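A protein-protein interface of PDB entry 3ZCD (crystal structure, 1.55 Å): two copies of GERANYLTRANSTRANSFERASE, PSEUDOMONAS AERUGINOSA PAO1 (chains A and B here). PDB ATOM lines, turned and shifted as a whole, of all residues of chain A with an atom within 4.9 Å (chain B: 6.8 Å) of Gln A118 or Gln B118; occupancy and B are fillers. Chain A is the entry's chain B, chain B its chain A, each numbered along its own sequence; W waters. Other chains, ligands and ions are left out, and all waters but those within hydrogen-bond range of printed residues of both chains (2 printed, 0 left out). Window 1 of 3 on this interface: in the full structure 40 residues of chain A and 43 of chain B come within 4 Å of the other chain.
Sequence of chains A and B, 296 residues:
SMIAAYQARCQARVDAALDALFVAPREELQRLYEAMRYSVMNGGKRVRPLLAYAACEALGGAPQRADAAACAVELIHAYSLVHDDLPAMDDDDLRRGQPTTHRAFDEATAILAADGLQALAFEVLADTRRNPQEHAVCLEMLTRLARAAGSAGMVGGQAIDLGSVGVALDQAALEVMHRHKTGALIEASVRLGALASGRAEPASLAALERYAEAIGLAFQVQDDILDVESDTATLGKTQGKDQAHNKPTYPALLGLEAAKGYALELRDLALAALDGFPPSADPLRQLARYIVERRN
Of the printed residues of chain B, Ala A119 touches Gln B118 (3.5 Å), Ala B146 (3.6 Å) and Gly B150 (3.6 Å).
Of the printed residues of chain A, His B83 touches Asp A115 (2.7 Å).
Gln B118 touches three residues of chain A.
Of the printed residues of chain A, Phe B122 touches Phe A122 (3.4 Å).
Of the printed residues of chain A, Gly B150 touches Ala A119 (3.6 Å).
The nearest residue of chain B that does not touch Gln A118 is Phe B122 (5.1 Å).
The nearest printed residue of chain A that does not touch Gln B118 is Phe A122 (5.2 Å).
O of Gly B150 is in hydrogen-bond range of N of Val B155 (3.2 Å).
Among the printed residues, merely in contact across the chains: Tyr A79 with Asp B115, Asp A115 with Tyr B79, Asp A115 with Asp B115, Gln A118 with Gln B118, Gln A118 with Ala B119, Ala A119 with Gln B118, Ala A119 with Ala B146, Ala A119 with Gly B150 and Phe A122 with Phe B122.
A ring nitrogen (ND1) of His B83 is in hydrogen-bond range of the side-chain carboxylate of Asp A115 (2.7 Å).
NE2 of Gln A118 lies within hydrogen-bond range of O of Asp B115, 3.2 Å away.
NE2 of Gln B118 lies within hydrogen-bond range of O of Asp A115 (3.2 Å).
Tyr A79 touches Asp B115, and with the chains exchanged Asp A115 touches Tyr B79.
Asp A115 touches its own counterpart, Asp B115.
Gln B118 touches its own counterpart, Gln A118.
Phe A122 touches its own counterpart, Phe B122.
Positions printed for both chains: 76, 79, 114, 115, 116, 117, 118, 119, 120, 121, 122 and 149.
Of the 12 pairs that touch across the chains among the printed residues, 9 have their exchanged pair printed and touching as well.
Water W2 lies within hydrogen-bond range of OD1 of Asp B115 (2.8 Å), OD1 of Asp A115 (2.8 Å), NE2 of Gln A118 (2.9 Å) and NE2 of Gln B118 (2.9 Å).
Water W1 bridges the backbone carbonyl oxygen (O) of Ala B146 and the backbone NH (N) of Leu A120.
Hydrophobic or aromatic side chains of chain A that line the printed part of chain B: Tyr A79, Ala A119 and Phe A122.
Of the 23 printed residues of chain B, 8 touch a printed residue of chain A.
Among the printed residues, 12 pairs touch across the chains.
Among the printed residues, no Asp or Glu carboxylate lies within 4 Å of a Lys or Arg side-chain nitrogen of the other chain.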
ATOM      1  N   ILE A  76      15.964 -14.664   4.553  1.00  0.00           N
ATOM      2  CA  ILE A  76      15.562 -15.087   5.883  1.00  0.00           C
ATOM      3  C   ILE A  76      14.677 -16.320   5.771  1.00  0.00           C
ATOM      4  O   ILE A  76      14.898 -17.322   6.471  1.00  0.00           O
ATOM      5  CB  ILE A  76      14.919 -14.000   6.752  1.00  0.00           C
ATOM      6  CG1 ILE A  76      15.935 -12.891   7.056  1.00  0.00           C
ATOM      7  CG2 ILE A  76      14.291 -14.576   8.005  1.00  0.00           C
ATOM      8  CD1 ILE A  76      17.108 -13.379   7.977  1.00  0.00           C
ATOM      9  N   TYR A  79      16.682 -19.390   4.544  1.00  0.00           N
ATOM     10  CA  TYR A  79      17.617 -19.987   5.564  1.00  0.00           C
ATOM     11  C   TYR A  79      16.769 -20.781   6.565  1.00  0.00           C
ATOM     12  O   TYR A  79      17.162 -21.929   6.938  1.00  0.00           O
ATOM     13  CB  TYR A  79      18.557 -18.972   6.235  1.00  0.00           C
ATOM     14  CG  TYR A  79      18.253 -18.741   7.719  1.00  0.00           C
ATOM     15  CD1 TYR A  79      18.531 -19.742   8.684  1.00  0.00           C
ATOM     16  CD2 TYR A  79      17.633 -17.571   8.177  1.00  0.00           C
ATOM     17  CE1 TYR A  79      18.231 -19.547   9.969  1.00  0.00           C
ATOM     18  CE2 TYR A  79      17.316 -17.379   9.512  1.00  0.00           C
ATOM     19  CZ  TYR A  79      17.649 -18.441  10.433  1.00  0.00           C
ATOM     20  OH  TYR A  79      17.283 -18.241  11.743  1.00  0.00           O
ATOM     21  N   ALA A 114      22.989 -21.966   5.266  1.00  0.00           N
ATOM     22  CA  ALA A 114      21.868 -21.225   5.830  1.00  0.00           C
ATOM     23  C   ALA A 114      22.342 -20.127   6.771  1.00  0.00           C
ATOM     24  O   ALA A 114      21.776 -19.024   6.819  1.00  0.00           O
ATOM     25  CB  ALA A 114      20.823 -22.110   6.445  1.00  0.00           C
ATOM     26  N   ASP A 115      23.346 -20.419   7.598  1.00  0.00           N
ATOM     27  CA  ASP A 115      23.944 -19.414   8.460  1.00  0.00           C
ATOM     28  C   ASP A 115      24.447 -18.210   7.649  1.00  0.00           C
ATOM     29  O   ASP A 115      24.239 -17.093   8.103  1.00  0.00           O
ATOM     30  CB  ASP A 115      25.093 -20.025   9.279  1.00  0.00           C
ATOM     31  CG  ASP A 115      24.601 -20.856  10.451  1.00  0.00           C
ATOM     32  OD1 ASP A 115      23.470 -20.833  10.847  1.00  0.00           O
ATOM     33  OD2 ASP A 115      25.539 -21.595  10.969  1.00  0.00           O
ATOM     34  N   GLY A 116      25.074 -18.497   6.516  1.00  0.00           N
ATOM     35  CA  GLY A 116      25.580 -17.473   5.586  1.00  0.00           C
ATOM     36  C   GLY A 116      24.476 -16.730   4.877  1.00  0.00           C
ATOM     37  O   GLY A 116      24.592 -15.497   4.711  1.00  0.00           O
ATOM     38  N   LEU A 117      23.381 -17.414   4.612  1.00  0.00           N
ATOM     39  CA  LEU A 117      22.173 -16.721   4.099  1.00  0.00           C
ATOM     40  C   LEU A 117      21.610 -15.726   5.065  1.00  0.00           C
ATOM     41  O   LEU A 117      21.128 -14.637   4.654  1.00  0.00           O
ATOM     42  CB  LEU A 117      21.084 -17.699   3.706  1.00  0.00           C
ATOM     43  CG  LEU A 117      21.391 -18.662   2.561  1.00  0.00           C
ATOM     44  CD1 LEU A 117      20.282 -19.648   2.379  1.00  0.00           C
ATOM     45  CD2 LEU A 117      21.683 -17.923   1.254  1.00  0.00           C
ATOM     46  N   GLN A 118      21.561 -16.036   6.352  1.00  0.00           N
ATOM     47  CA  GLN A 118      21.060 -15.116   7.328  1.00  0.00           C
ATOM     48  C   GLN A 118      21.967 -13.890   7.361  1.00  0.00           C
ATOM     49  O   GLN A 118      21.448 -12.752   7.396  1.00  0.00           O
ATOM     50  CB  GLN A 118      20.910 -15.737   8.778  1.00  0.00           C
ATOM     51  CG  GLN A 118      20.322 -14.697   9.712  1.00  0.00           C
ATOM     52  CD  GLN A 118      19.736 -15.066  11.035  1.00  0.00           C
ATOM     53  OE1 GLN A 118      18.972 -14.331  11.617  1.00  0.00           O
ATOM     54  NE2 GLN A 118      20.192 -16.227  11.605  1.00  0.00           N
ATOM     55  N   ALA A 119      23.276 -14.037   7.452  1.00  0.00           N
ATOM     56  CA  ALA A 119      24.216 -12.917   7.471  1.00  0.00           C
ATOM     57  C   ALA A 119      23.948 -12.059   6.234  1.00  0.00           C
ATOM     58  O   ALA A 119      23.957 -10.816   6.365  1.00  0.00           O
ATOM     59  CB  ALA A 119      25.668 -13.380   7.508  1.00  0.00           C
ATOM     60  N   LEU A 120      23.783 -12.742   5.119  1.00  0.00           N
ATOM     61  CA  LEU A 120      23.637 -12.030   3.800  1.00  0.00           C
ATOM     62  C   LEU A 120      22.399 -11.205   3.837  1.00  0.00           C
ATOM     63  O   LEU A 120      22.390 -10.129   3.176  1.00  0.00           O
ATOM     64  CB  LEU A 120      23.569 -13.021   2.673  1.00  0.00           C
ATOM     65  CG  LEU A 120      23.530 -12.536   1.216  1.00  0.00           C
ATOM     66  CD1 LEU A 120      24.683 -11.630   0.924  1.00  0.00           C
ATOM     67  CD2 LEU A 120      23.554 -13.759   0.328  1.00  0.00           C
ATOM     68  N   ALA A 121      21.334 -11.655   4.454  1.00  0.00           N
ATOM     69  CA  ALA A 121      20.078 -10.856   4.531  1.00  0.00           C
ATOM     70  C   ALA A 121      20.347  -9.504   5.149  1.00  0.00           C
ATOM     71  O   ALA A 121      19.859  -8.468   4.632  1.00  0.00           O
ATOM     72  CB  ALA A 121      18.959 -11.566   5.260  1.00  0.00           C
ATOM     73  N   PHE A 122      21.087  -9.438   6.245  1.00  0.00           N
ATOM     74  CA  PHE A 122      21.420  -8.196   6.913  1.00  0.00           C
ATOM     75  C   PHE A 122      22.415  -7.391   6.089  1.00  0.00           C
ATOM     76  O   PHE A 122      22.340  -6.156   6.052  1.00  0.00           O
ATOM     77  CB  PHE A 122      21.890  -8.496   8.356  1.00  0.00           C
ATOM     78  CG  PHE A 122      20.771  -9.049   9.166  1.00  0.00           C
ATOM     79  CD1 PHE A 122      19.702  -8.287   9.580  1.00  0.00           C
ATOM     80  CD2 PHE A 122      20.767 -10.397   9.516  1.00  0.00           C
ATOM     81  CE1 PHE A 122      18.624  -8.810  10.245  1.00  0.00           C
ATOM     82  CE2 PHE A 122      19.722 -10.924  10.267  1.00  0.00           C
ATOM     83  CZ  PHE A 122      18.654 -10.162  10.648  1.00  0.00           C
ATOM     84  N   ALA A 149      12.994 -11.802  12.564  1.00  0.00           N
ATOM     85  CA  ALA A 149      13.689 -13.029  12.233  1.00  0.00           C
ATOM     86  C   ALA A 149      14.179 -13.759  13.481  1.00  0.00           C
ATOM     87  O   ALA A 149      14.370 -14.999  13.388  1.00  0.00           O
ATOM     88  CB  ALA A 149      14.878 -12.772  11.341  1.00  0.00           C
ATOM     89  N   ALA B  72      27.848  -7.482  19.880  1.00  0.00           N
ATOM     90  CA  ALA B  72      27.595  -8.092  18.606  1.00  0.00           C
ATOM     91  C   ALA B  72      28.652  -9.142  18.181  1.00  0.00           C
ATOM     92  O   ALA B  72      28.299 -10.217  17.717  1.00  0.00           O
ATOM     93  CB  ALA B  72      27.437  -6.982  17.537  1.00  0.00           C
ATOM     94  N   LEU B  75      28.253 -12.216  20.319  1.00  0.00           N
ATOM     95  CA  LEU B  75      27.069 -12.954  19.914  1.00  0.00           C
ATOM     96  C   LEU B  75      27.332 -13.796  18.670  1.00  0.00           C
ATOM     97  O   LEU B  75      26.876 -14.962  18.564  1.00  0.00           O
ATOM     98  CB  LEU B  75      25.877 -12.007  19.682  1.00  0.00           C
ATOM     99  CG  LEU B  75      25.291 -11.433  20.976  1.00  0.00           C
ATOM    100  CD1 LEU B  75      24.395 -10.220  20.662  1.00  0.00           C
ATOM    101  CD2 LEU B  75      24.460 -12.438  21.731  1.00  0.00           C
ATOM    102  N   ILE B  76      28.016 -13.192  17.679  1.00  0.00           N
ATOM    103  CA  ILE B  76      28.428 -13.921  16.506  1.00  0.00           C
ATOM    104  C   ILE B  76      29.338 -15.110  16.911  1.00  0.00           C
ATOM    105  O   ILE B  76      29.111 -16.218  16.464  1.00  0.00           O
ATOM    106  CB  ILE B  76      29.075 -13.055  15.420  1.00  0.00           C
ATOM    107  CG1 ILE B  76      28.054 -12.046  14.857  1.00  0.00           C
ATOM    108  CG2 ILE B  76      29.717 -13.898  14.326  1.00  0.00           C
ATOM    109  CD1 ILE B  76      26.917 -12.669  14.099  1.00  0.00           C
ATOM    110  N   TYR B  79      27.242 -17.867  18.736  1.00  0.00           N
ATOM    111  CA  TYR B  79      26.409 -18.687  17.943  1.00  0.00           C
ATOM    112  C   TYR B  79      27.266 -19.686  17.109  1.00  0.00           C
ATOM    113  O   TYR B  79      26.861 -20.848  16.917  1.00  0.00           O
ATOM    114  CB  TYR B  79      25.469 -17.772  17.024  1.00  0.00           C
ATOM    115  CG  TYR B  79      25.771 -17.867  15.513  1.00  0.00           C
ATOM    116  CD1 TYR B  79      25.410 -18.944  14.771  1.00  0.00           C
ATOM    117  CD2 TYR B  79      26.374 -16.820  14.844  1.00  0.00           C
ATOM    118  CE1 TYR B  79      25.782 -19.112  13.455  1.00  0.00           C
ATOM    119  CE2 TYR B  79      26.663 -16.893  13.480  1.00  0.00           C
ATOM    120  CZ  TYR B  79      26.368 -18.021  12.768  1.00  0.00           C
ATOM    121  OH  TYR B  79      26.717 -18.197  11.462  1.00  0.00           O
ATOM    122  N   HIS B  83      26.773 -23.914  16.859  1.00  0.00           N
ATOM    123  CA  HIS B  83      26.650 -24.687  15.665  1.00  0.00           C
ATOM    124  C   HIS B  83      27.855 -25.622  15.406  1.00  0.00           C
ATOM    125  O   HIS B  83      27.669 -26.721  14.934  1.00  0.00           O
ATOM    126  CB  HIS B  83      26.400 -23.791  14.427  1.00  0.00           C
ATOM    127  CG  HIS B  83      24.993 -23.303  14.340  1.00  0.00           C
ATOM    128  ND1 HIS B  83      24.536 -22.516  13.272  1.00  0.00           N
ATOM    129  CD2 HIS B  83      23.932 -23.493  15.138  1.00  0.00           C
ATOM    130  CE1 HIS B  83      23.261 -22.251  13.451  1.00  0.00           C
ATOM    131  NE2 HIS B  83      22.863 -22.803  14.586  1.00  0.00           N
ATOM    132  N   LEU B 112      18.357 -23.472  16.870  1.00  0.00           N
ATOM    133  CA  LEU B 112      17.458 -22.268  16.937  1.00  0.00           C
ATOM    134  C   LEU B 112      18.008 -21.164  17.821  1.00  0.00           C
ATOM    135  O   LEU B 112      18.038 -19.942  17.427  1.00  0.00           O
ATOM    136  CB  LEU B 112      16.074 -22.636  17.383  1.00  0.00           C
ATOM    137  CG  LEU B 112      15.279 -23.457  16.405  1.00  0.00           C
ATOM    138  CD1 LEU B 112      13.991 -23.962  16.978  1.00  0.00           C
ATOM    139  CD2 LEU B 112      14.925 -22.612  15.142  1.00  0.00           C
ATOM    140  N   ALA B 113      18.491 -21.520  19.047  1.00  0.00           N
ATOM    141  CA  ALA B 113      19.022 -20.529  19.932  1.00  0.00           C
ATOM    142  C   ALA B 113      20.152 -19.770  19.205  1.00  0.00           C
ATOM    143  O   ALA B 113      20.244 -18.527  19.282  1.00  0.00           O
ATOM    144  CB  ALA B 113      19.548 -21.211  21.231  1.00  0.00           C
ATOM    145  N   ALA B 114      21.048 -20.515  18.556  1.00  0.00           N
ATOM    146  CA  ALA B 114      22.189 -19.926  17.869  1.00  0.00           C
ATOM    147  C   ALA B 114      21.699 -19.046  16.667  1.00  0.00           C
ATOM    148  O   ALA B 114      22.280 -17.997  16.450  1.00  0.00           O
ATOM    149  CB  ALA B 114      23.200 -21.000  17.457  1.00  0.00           C
ATOM    150  N   ASP B 115      20.679 -19.519  15.986  1.00  0.00           N
ATOM    151  CA  ASP B 115      20.078 -18.714  14.856  1.00  0.00           C
ATOM    152  C   ASP B 115      19.580 -17.398  15.403  1.00  0.00           C
ATOM    153  O   ASP B 115      19.838 -16.344  14.750  1.00  0.00           O
ATOM    154  CB  ASP B 115      18.958 -19.483  14.218  1.00  0.00           C
ATOM    155  CG  ASP B 115      19.423 -20.601  13.285  1.00  0.00           C
ATOM    156  OD1 ASP B 115      20.555 -20.565  12.871  1.00  0.00           O
ATOM    157  OD2 ASP B 115      18.594 -21.461  12.882  1.00  0.00           O
ATOM    158  N   GLY B 116      18.935 -17.402  16.549  1.00  0.00           N
ATOM    159  CA  GLY B 116      18.425 -16.205  17.233  1.00  0.00           C
ATOM    160  C   GLY B 116      19.545 -15.297  17.701  1.00  0.00           C
ATOM    161  O   GLY B 116      19.422 -14.069  17.734  1.00  0.00           O
ATOM    162  N   LEU B 117      20.659 -15.924  18.195  1.00  0.00           N
ATOM    163  CA  LEU B 117      21.837 -15.149  18.574  1.00  0.00           C
ATOM    164  C   LEU B 117      22.400 -14.337  17.382  1.00  0.00           C
ATOM    165  O   LEU B 117      22.894 -13.251  17.597  1.00  0.00           O
ATOM    166  CB  LEU B 117      22.973 -16.033  19.164  1.00  0.00           C
ATOM    167  CG  LEU B 117      22.591 -16.637  20.504  1.00  0.00           C
ATOM    168  CD1 LEU B 117      23.722 -17.617  20.928  1.00  0.00           C
ATOM    169  CD2 LEU B 117      22.327 -15.684  21.646  1.00  0.00           C
ATOM    170  N   GLN B 118      22.433 -14.963  16.216  1.00  0.00           N
ATOM    171  CA  GLN B 118      22.951 -14.273  15.002  1.00  0.00           C
ATOM    172  C   GLN B 118      22.050 -13.058  14.719  1.00  0.00           C
ATOM    173  O   GLN B 118      22.572 -11.956  14.547  1.00  0.00           O
ATOM    174  CB  GLN B 118      23.084 -15.143  13.771  1.00  0.00           C
ATOM    175  CG  GLN B 118      23.708 -14.315  12.658  1.00  0.00           C
ATOM    176  CD  GLN B 118      24.233 -15.000  11.418  1.00  0.00           C
ATOM    177  OE1 GLN B 118      25.091 -14.443  10.757  1.00  0.00           O
ATOM    178  NE2 GLN B 118      23.734 -16.172  11.091  1.00  0.00           N
ATOM    179  N   ALA B 119      20.753 -13.286  14.680  1.00  0.00           N
ATOM    180  CA  ALA B 119      19.777 -12.146  14.462  1.00  0.00           C
ATOM    181  C   ALA B 119      19.991 -11.042  15.485  1.00  0.00           C
ATOM    182  O   ALA B 119      20.037  -9.809  15.129  1.00  0.00           O
ATOM    183  CB  ALA B 119      18.373 -12.606  14.497  1.00  0.00           C
ATOM    184  N   LEU B 120      20.189 -11.412  16.763  1.00  0.00           N
ATOM    185  CA  LEU B 120      20.363 -10.480  17.852  1.00  0.00           C
ATOM    186  C   LEU B 120      21.640  -9.634  17.678  1.00  0.00           C
ATOM    187  O   LEU B 120      21.653  -8.483  18.084  1.00  0.00           O
ATOM    188  CB  LEU B 120      20.435 -11.268  19.187  1.00  0.00           C
ATOM    189  CG  LEU B 120      20.453 -10.459  20.472  1.00  0.00           C
ATOM    190  CD1 LEU B 120      19.275  -9.504  20.592  1.00  0.00           C
ATOM    191  CD2 LEU B 120      20.427 -11.418  21.643  1.00  0.00           C
ATOM    192  N   ALA B 121      22.727 -10.232  17.161  1.00  0.00           N
ATOM    193  CA  ALA B 121      23.970  -9.502  16.913  1.00  0.00           C
ATOM    194  C   ALA B 121      23.656  -8.261  15.970  1.00  0.00           C
ATOM    195  O   ALA B 121      24.134  -7.186  16.227  1.00  0.00           O
ATOM    196  CB  ALA B 121      25.061 -10.360  16.306  1.00  0.00           C
ATOM    197  N   PHE B 122      22.895  -8.531  14.937  1.00  0.00           N
ATOM    198  CA  PHE B 122      22.559  -7.465  13.990  1.00  0.00           C
ATOM    199  C   PHE B 122      21.541  -6.507  14.575  1.00  0.00           C
ATOM    200  O   PHE B 122      21.667  -5.263  14.394  1.00  0.00           O
ATOM    201  CB  PHE B 122      22.117  -8.061  12.682  1.00  0.00           C
ATOM    202  CG  PHE B 122      23.200  -8.808  12.004  1.00  0.00           C
ATOM    203  CD1 PHE B 122      24.331  -8.169  11.578  1.00  0.00           C
ATOM    204  CD2 PHE B 122      23.168 -10.189  11.898  1.00  0.00           C
ATOM    205  CE1 PHE B 122      25.403  -8.821  10.978  1.00  0.00           C
ATOM    206  CE2 PHE B 122      24.226 -10.833  11.270  1.00  0.00           C
ATOM    207  CZ  PHE B 122      25.359 -10.170  10.860  1.00  0.00           C
ATOM    208  N   GLU B 123      20.558  -7.031  15.298  1.00  0.00           N
ATOM    209  CA  GLU B 123      19.645  -6.193  16.081  1.00  0.00           C
ATOM    210  C   GLU B 123      20.379  -5.144  16.921  1.00  0.00           C
ATOM    211  O   GLU B 123      20.071  -3.961  16.925  1.00  0.00           O
ATOM    212  CB  GLU B 123      18.725  -7.028  16.967  1.00  0.00           C
ATOM    213  CG  GLU B 123      17.679  -6.193  17.674  1.00  0.00           C
ATOM    214  CD  GLU B 123      16.826  -6.993  18.644  1.00  0.00           C
ATOM    215  OE1 GLU B 123      16.514  -8.149  18.302  1.00  0.00           O
ATOM    216  OE2 GLU B 123      16.445  -6.435  19.704  1.00  0.00           O
ATOM    217  N   LEU B 145      30.287  -6.310   9.906  1.00  0.00           N
ATOM    218  CA  LEU B 145      30.005  -7.551  10.722  1.00  0.00           C
ATOM    219  C   LEU B 145      29.356  -8.594   9.859  1.00  0.00           C
ATOM    220  O   LEU B 145      29.683  -9.783   9.901  1.00  0.00           O
ATOM    221  CB  LEU B 145      29.103  -7.273  11.910  1.00  0.00           C
ATOM    222  CG  LEU B 145      29.039  -8.537  12.838  1.00  0.00           C
ATOM    223  CD1 LEU B 145      30.398  -9.047  13.319  1.00  0.00           C
ATOM    224  CD2 LEU B 145      28.175  -8.241  14.036  1.00  0.00           C
ATOM    225  N   ALA B 146      28.395  -8.193   9.014  1.00  0.00           N
ATOM    226  CA  ALA B 146      27.720  -9.148   8.141  1.00  0.00           C
ATOM    227  C   ALA B 146      28.700  -9.856   7.169  1.00  0.00           C
ATOM    228  O   ALA B 146      28.603 -11.063   6.921  1.00  0.00           O
ATOM    229  CB  ALA B 146      26.561  -8.476   7.339  1.00  0.00           C
ATOM    230  N   ALA B 149      31.025 -12.088   9.226  1.00  0.00           N
ATOM    231  CA  ALA B 149      30.323 -13.269   9.805  1.00  0.00           C
ATOM    232  C   ALA B 149      29.856 -14.283   8.785  1.00  0.00           C
ATOM    233  O   ALA B 149      29.703 -15.482   9.117  1.00  0.00           O
ATOM    234  CB  ALA B 149      29.165 -12.843  10.648  1.00  0.00           C
ATOM    235  N   GLY B 150      29.586 -13.839   7.548  1.00  0.00           N
ATOM    236  CA  GLY B 150      28.925 -14.643   6.574  1.00  0.00           C
ATOM    237  C   GLY B 150      29.817 -15.574   5.787  1.00  0.00           C
ATOM    238  O   GLY B 150      30.963 -15.873   6.184  1.00  0.00           O
ATOM    239  N   MET B 154      33.594 -15.747   8.291  1.00  0.00           N
ATOM    240  CA  MET B 154      33.692 -16.800   9.348  1.00  0.00           C
ATOM    241  C   MET B 154      33.058 -18.089   8.856  1.00  0.00           C
ATOM    242  O   MET B 154      33.673 -19.197   8.956  1.00  0.00           O
ATOM    243  CB  MET B 154      32.971 -16.304  10.577  1.00  0.00           C
ATOM    244  CG  MET B 154      32.899 -17.316  11.738  1.00  0.00           C
ATOM    245  SD  MET B 154      31.925 -16.751  13.102  1.00  0.00           S
ATOM    246  CE  MET B 154      30.281 -16.978  12.407  1.00  0.00           C
ATOM    247  N   VAL B 155      31.826 -18.018   8.351  1.00  0.00           N
ATOM    248  CA  VAL B 155      31.136 -19.188   7.850  1.00  0.00           C
ATOM    249  C   VAL B 155      31.926 -19.819   6.685  1.00  0.00           C
ATOM    250  O   VAL B 155      32.007 -21.033   6.569  1.00  0.00           O
ATOM    251  CB  VAL B 155      29.686 -18.882   7.461  1.00  0.00           C
ATOM    252  CG1 VAL B 155      29.064 -19.957   6.585  1.00  0.00           C
ATOM    253  CG2 VAL B 155      28.861 -18.637   8.708  1.00  0.00           C
HETATM  254  O   HOH W   1      27.062 -11.829   4.642  1.00  0.00           O
HETATM  255  O   HOH W   2      22.023 -18.515  11.621  1.00  0.00           O
